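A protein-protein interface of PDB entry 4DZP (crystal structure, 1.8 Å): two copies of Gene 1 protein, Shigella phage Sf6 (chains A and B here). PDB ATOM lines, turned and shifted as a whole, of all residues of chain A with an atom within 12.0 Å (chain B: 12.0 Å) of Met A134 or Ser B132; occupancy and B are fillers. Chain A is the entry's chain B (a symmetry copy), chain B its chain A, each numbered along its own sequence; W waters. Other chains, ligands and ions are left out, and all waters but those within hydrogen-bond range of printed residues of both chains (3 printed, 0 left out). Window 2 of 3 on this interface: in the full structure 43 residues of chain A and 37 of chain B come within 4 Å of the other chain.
Of chain B, only Glu B130 and Ser B132 come within 4 Å of Met A134. Ser B132 touches two residues of chain A. Ser A132 touches just these residues of chain B: Ile B129, Glu B130 and Thr B131. Of chain B, only Glu B130 comes within 4 Å of Pro A133. Of chain B, only Glu B130 (2.8 Å) comes within 4 Å of Ser A135. Leu A137 touches none of the printed residues of chain B. Of chain B, only Glu B130 and Ser B132 come within 4 Å of Phe A138. No residue of chain B comes within 4 Å of Gly A139. Glu B130 touches just these residues of chain A: Ser A132 (3.3 Å), Pro A133 (3.5 Å), Met A134 (3.3 Å), Ser A135 (2.8 Å) and Phe A138 (3.6 Å). Of chain A, only Ser A132 (3.6 Å) comes within 4 Å of Thr B131. Printed residues of chain B within 4 Å of Thr A131: Ile B129. Printed residues of chain A within 4 Å of Gln B128: Glu A130 (2.9 Å). Of the printed residues of chain B, Glu A130 touches Gln B128 and Ile B129. The nearest printed residue of chain B that does not touch Thr A131 is Thr B131 (5.4 Å).
The side-chain hydroxyl (OG) of Ser B132 is in hydrogen-bond range of the side-chain sulfur (SD) of Met A134 (3.4 Å). The backbone carbonyl oxygen (O) of Glu A130 is in hydrogen-bond range of the backbone NH (N) of Ile B129 (2.9 Å). The backbone carbonyl oxygen (O) of Ile B129 is in hydrogen-bond range of the backbone NH (N) of Ser A132 (2.9 Å). The side-chain amide oxygen of Gln B128 sits close to the side-chain carboxylate of Glu A130 (2.9 Å). OE2 of Glu B130 lies within hydrogen-bond range of OG of Ser A135, at 2.8 Å.
Ile B129 touches Thr A131 (O to CA, 3.3 Å). Ser A132 touches Glu B130 (O to CA, 3.3 Å). Thr B131 touches Ser A132. Glu B130 touches Pro A133. Glu B130 touches Met A134 (OE1 to CA, 3.3 Å). Phe A138 touches Glu B130 (CE2 to OE1, 3.6 Å). Phe A138 touches Ser B132 (CE1 to OG, 2.8 Å).
Ser A132 touches Glu B130, but with the chains exchanged Glu A130 does not touch Ser B132 (11.4 Å). Ser A132 touches Thr B131, but with the chains exchanged Thr A131 does not touch Ser B132 (9.2 Å). 3 positions are printed for both chains. Of the 12 pairs that touch across the chains among the printed residues, none has its exchanged pair printed and touching as well.
Water W3 lies within hydrogen-bond range of the side-chain amide nitrogen of Gln B128, the side-chain hydroxyl of Ser A132, the backbone carbonyl oxygen of Glu A130 and the backbone carbonyl oxygen of Ile B129. Water W2 lies within hydrogen-bond range of the side-chain carboxylate of Glu B130 (2.8 Å), the side-chain hydroxyl of Thr A136 (2.9 Å) and the side-chain hydroxyl of Ser A135 (3.3 Å). Water W1 lies within hydrogen-bond range of OE2 of Glu B130 (3.0 Å) and OG of Ser A135 (3.5 Å).
Of the 5 printed residues of chain B, 5 touch a printed residue of chain A. Of the 10 printed residues of chain A, 7 touch a printed residue of chain B. Printed residues of chain A that touch a printed residue of chain B: Glu A130, Thr A131, Ser A132, Pro A133, Met A134, Ser A135 and Phe A138. Among the printed residues, 12 pairs touch across the chains.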
ATOM      1  N   GLU A 130       0.060  -4.886  26.483  1.00  0.00           N
ATOM      2  CA  GLU A 130      -0.436  -5.787  25.457  1.00  0.00           C
ATOM      3  C   GLU A 130      -1.406  -6.760  26.097  1.00  0.00           C
ATOM      4  O   GLU A 130      -1.042  -7.480  27.026  1.00  0.00           O
ATOM      5  CB  GLU A 130       0.722  -6.555  24.834  1.00  0.00           C
ATOM      6  CG  GLU A 130       0.300  -7.581  23.814  1.00  0.00           C
ATOM      7  CD  GLU A 130       1.466  -8.081  22.982  1.00  0.00           C
ATOM      8  OE1 GLU A 130       1.217  -8.837  22.020  1.00  0.00           O
ATOM      9  OE2 GLU A 130       2.624  -7.714  23.285  1.00  0.00           O
ATOM     10  N   THR A 131      -2.646  -6.768  25.617  1.00  0.00           N
ATOM     11  CA  THR A 131      -3.649  -7.667  26.164  1.00  0.00           C
ATOM     12  C   THR A 131      -3.818  -8.871  25.247  1.00  0.00           C
ATOM     13  O   THR A 131      -3.707  -8.753  24.028  1.00  0.00           O
ATOM     14  CB  THR A 131      -5.011  -6.973  26.352  1.00  0.00           C
ATOM     15  OG1 THR A 131      -5.433  -6.397  25.110  1.00  0.00           O
ATOM     16  CG2 THR A 131      -4.924  -5.885  27.413  1.00  0.00           C
ATOM     17  N   SER A 132      -4.074 -10.030  25.844  1.00  0.00           N
ATOM     18  CA  SER A 132      -4.226 -11.270  25.097  1.00  0.00           C
ATOM     19  C   SER A 132      -5.363 -12.067  25.710  1.00  0.00           C
ATOM     20  O   SER A 132      -5.748 -11.826  26.855  1.00  0.00           O
ATOM     21  CB  SER A 132      -2.937 -12.095  25.151  1.00  0.00           C
ATOM     22  OG  SER A 132      -1.926 -11.535  24.333  1.00  0.00           O
ATOM     23  N   PRO A 133      -5.926 -13.007  24.941  1.00  0.00           N
ATOM     24  CA  PRO A 133      -6.945 -13.886  25.526  1.00  0.00           C
ATOM     25  C   PRO A 133      -6.284 -14.817  26.538  1.00  0.00           C
ATOM     26  O   PRO A 133      -5.091 -15.096  26.416  1.00  0.00           O
ATOM     27  CB  PRO A 133      -7.453 -14.690  24.324  1.00  0.00           C
ATOM     28  CG  PRO A 133      -6.988 -13.935  23.103  1.00  0.00           C
ATOM     29  CD  PRO A 133      -5.708 -13.274  23.510  1.00  0.00           C
ATOM     30  N   MET A 134      -7.035 -15.295  27.523  1.00  0.00           N
ATOM     31  CA  MET A 134      -6.445 -16.195  28.509  1.00  0.00           C
ATOM     32  C   MET A 134      -5.798 -17.400  27.827  1.00  0.00           C
ATOM     33  O   MET A 134      -6.319 -17.931  26.844  1.00  0.00           O
ATOM     34  CB  MET A 134      -7.472 -16.605  29.571  1.00  0.00           C
ATOM     35  CG  MET A 134      -8.808 -17.044  29.017  1.00  0.00           C
ATOM     36  SD  MET A 134     -10.106 -17.001  30.270  1.00  0.00           S
ATOM     37  CE  MET A 134      -9.388 -18.021  31.552  1.00  0.00           C
ATOM     38  N   SER A 135      -4.640 -17.809  28.328  1.00  0.00           N
ATOM     39  CA  SER A 135      -3.925 -18.939  27.756  1.00  0.00           C
ATOM     40  C   SER A 135      -3.989 -20.156  28.676  1.00  0.00           C
ATOM     41  O   SER A 135      -3.560 -21.246  28.308  1.00  0.00           O
ATOM     42  CB  SER A 135      -2.469 -18.567  27.473  1.00  0.00           C
ATOM     43  OG  SER A 135      -1.803 -18.257  28.678  1.00  0.00           O
ATOM     44  N   THR A 136      -4.518 -19.948  29.877  1.00  0.00           N
ATOM     45  CA  THR A 136      -4.755 -21.022  30.842  1.00  0.00           C
ATOM     46  C   THR A 136      -6.098 -20.788  31.513  1.00  0.00           C
ATOM     47  O   THR A 136      -6.655 -19.692  31.434  1.00  0.00           O
ATOM     48  CB  THR A 136      -3.679 -21.059  31.934  1.00  0.00           C
ATOM     49  OG1 THR A 136      -3.778 -19.878  32.745  1.00  0.00           O
ATOM     50  CG2 THR A 136      -2.293 -21.142  31.319  1.00  0.00           C
ATOM     51  N   LEU A 137      -6.615 -21.815  32.185  1.00  0.00           N
ATOM     52  CA  LEU A 137      -7.898 -21.729  32.869  1.00  0.00           C
ATOM     53  C   LEU A 137      -7.751 -21.132  34.259  1.00  0.00           C
ATOM     54  O   LEU A 137      -7.652 -21.869  35.241  1.00  0.00           O
ATOM     55  CB  LEU A 137      -8.514 -23.127  33.000  1.00  0.00           C
ATOM     56  CG  LEU A 137      -9.343 -23.642  31.829  1.00  0.00           C
ATOM     57  CD1 LEU A 137      -9.581 -25.149  31.964  1.00  0.00           C
ATOM     58  CD2 LEU A 137     -10.668 -22.905  31.785  1.00  0.00           C
ATOM     59  N   PHE A 138      -7.759 -19.806  34.360  1.00  0.00           N
ATOM     60  CA  PHE A 138      -7.597 -19.169  35.665  1.00  0.00           C
ATOM     61  C   PHE A 138      -8.875 -18.537  36.217  1.00  0.00           C
ATOM     62  O   PHE A 138      -8.878 -17.988  37.318  1.00  0.00           O
ATOM     63  CB  PHE A 138      -6.444 -18.158  35.654  1.00  0.00           C
ATOM     64  CG  PHE A 138      -6.616 -17.025  34.678  1.00  0.00           C
ATOM     65  CD1 PHE A 138      -7.548 -16.021  34.907  1.00  0.00           C
ATOM     66  CD2 PHE A 138      -5.798 -16.930  33.559  1.00  0.00           C
ATOM     67  CE1 PHE A 138      -7.675 -14.957  34.025  1.00  0.00           C
ATOM     68  CE2 PHE A 138      -5.926 -15.866  32.672  1.00  0.00           C
ATOM     69  CZ  PHE A 138      -6.858 -14.885  32.906  1.00  0.00           C
ATOM     70  N   GLY A 139      -9.959 -18.628  35.455  1.00  0.00           N
ATOM     71  CA  GLY A 139     -11.237 -18.071  35.870  1.00  0.00           C
ATOM     72  C   GLY A 139     -11.861 -18.785  37.056  1.00  0.00           C
ATOM     73  O   GLY A 139     -11.283 -19.704  37.642  1.00  0.00           O
ATOM     74  N   GLN B 128       2.414  -7.677  29.657  1.00  0.00           N
ATOM     75  CA  GLN B 128       1.459  -8.667  29.144  1.00  0.00           C
ATOM     76  C   GLN B 128       0.316  -8.938  30.121  1.00  0.00           C
ATOM     77  O   GLN B 128       0.539  -9.354  31.259  1.00  0.00           O
ATOM     78  CB  GLN B 128       2.185  -9.986  28.850  1.00  0.00           C
ATOM     79  CG  GLN B 128       3.396  -9.838  27.925  1.00  0.00           C
ATOM     80  CD  GLN B 128       2.998  -9.423  26.519  1.00  0.00           C
ATOM     81  OE1 GLN B 128       3.613  -8.539  25.916  1.00  0.00           O
ATOM     82  NE2 GLN B 128       1.958 -10.058  25.994  1.00  0.00           N
ATOM     83  N   ILE B 129      -0.916  -8.732  29.664  1.00  0.00           N
ATOM     84  CA  ILE B 129      -2.070  -8.989  30.504  1.00  0.00           C
ATOM     85  C   ILE B 129      -3.019  -9.940  29.778  1.00  0.00           C
ATOM     86  O   ILE B 129      -3.195  -9.826  28.565  1.00  0.00           O
ATOM     87  CB  ILE B 129      -2.811  -7.680  30.802  1.00  0.00           C
ATOM     88  CG1 ILE B 129      -1.886  -6.710  31.570  1.00  0.00           C
ATOM     89  CG2 ILE B 129      -4.077  -7.945  31.584  1.00  0.00           C
ATOM     90  CD1 ILE B 129      -2.544  -5.385  31.921  1.00  0.00           C
ATOM     91  N   GLU B 130      -3.600 -10.882  30.517  1.00  0.00           N
ATOM     92  CA  GLU B 130      -4.676 -11.721  29.996  1.00  0.00           C
ATOM     93  C   GLU B 130      -5.907 -11.449  30.843  1.00  0.00           C
ATOM     94  O   GLU B 130      -5.818 -11.412  32.066  1.00  0.00           O
ATOM     95  CB  GLU B 130      -4.299 -13.212  30.082  1.00  0.00           C
ATOM     96  CG  GLU B 130      -3.278 -13.645  29.047  1.00  0.00           C
ATOM     97  CD  GLU B 130      -2.807 -15.065  29.261  1.00  0.00           C
ATOM     98  OE1 GLU B 130      -3.490 -15.810  29.995  1.00  0.00           O
ATOM     99  OE2 GLU B 130      -1.753 -15.433  28.701  1.00  0.00           O
ATOM    100  N   THR B 131      -7.060 -11.264  30.209  1.00  0.00           N
ATOM    101  CA  THR B 131      -8.285 -11.020  30.978  1.00  0.00           C
ATOM    102  C   THR B 131      -9.330 -12.097  30.703  1.00  0.00           C
ATOM    103  O   THR B 131      -9.391 -12.640  29.602  1.00  0.00           O
ATOM    104  CB  THR B 131      -8.874  -9.639  30.648  1.00  0.00           C
ATOM    105  OG1 THR B 131      -7.899  -8.622  30.924  1.00  0.00           O
ATOM    106  CG2 THR B 131     -10.117  -9.369  31.487  1.00  0.00           C
ATOM    107  N   SER B 132     -10.142 -12.420  31.704  1.00  0.00           N
ATOM    108  CA  SER B 132     -11.255 -13.334  31.477  1.00  0.00           C
ATOM    109  C   SER B 132     -12.528 -12.548  31.185  1.00  0.00           C
ATOM    110  O   SER B 132     -13.592 -12.825  31.743  1.00  0.00           O
ATOM    111  CB  SER B 132     -11.467 -14.244  32.679  1.00  0.00           C
ATOM    112  OG  SER B 132     -10.271 -14.941  32.968  1.00  0.00           O
HETATM  113  O   HOH W   1       0.638 -16.356  30.250  1.00  0.00           O
HETATM  114  O   HOH W   2      -2.297 -17.480  31.886  1.00  0.00           O
HETATM  115  O   HOH W   3      -0.663 -10.513  26.592  1.00  0.00           O
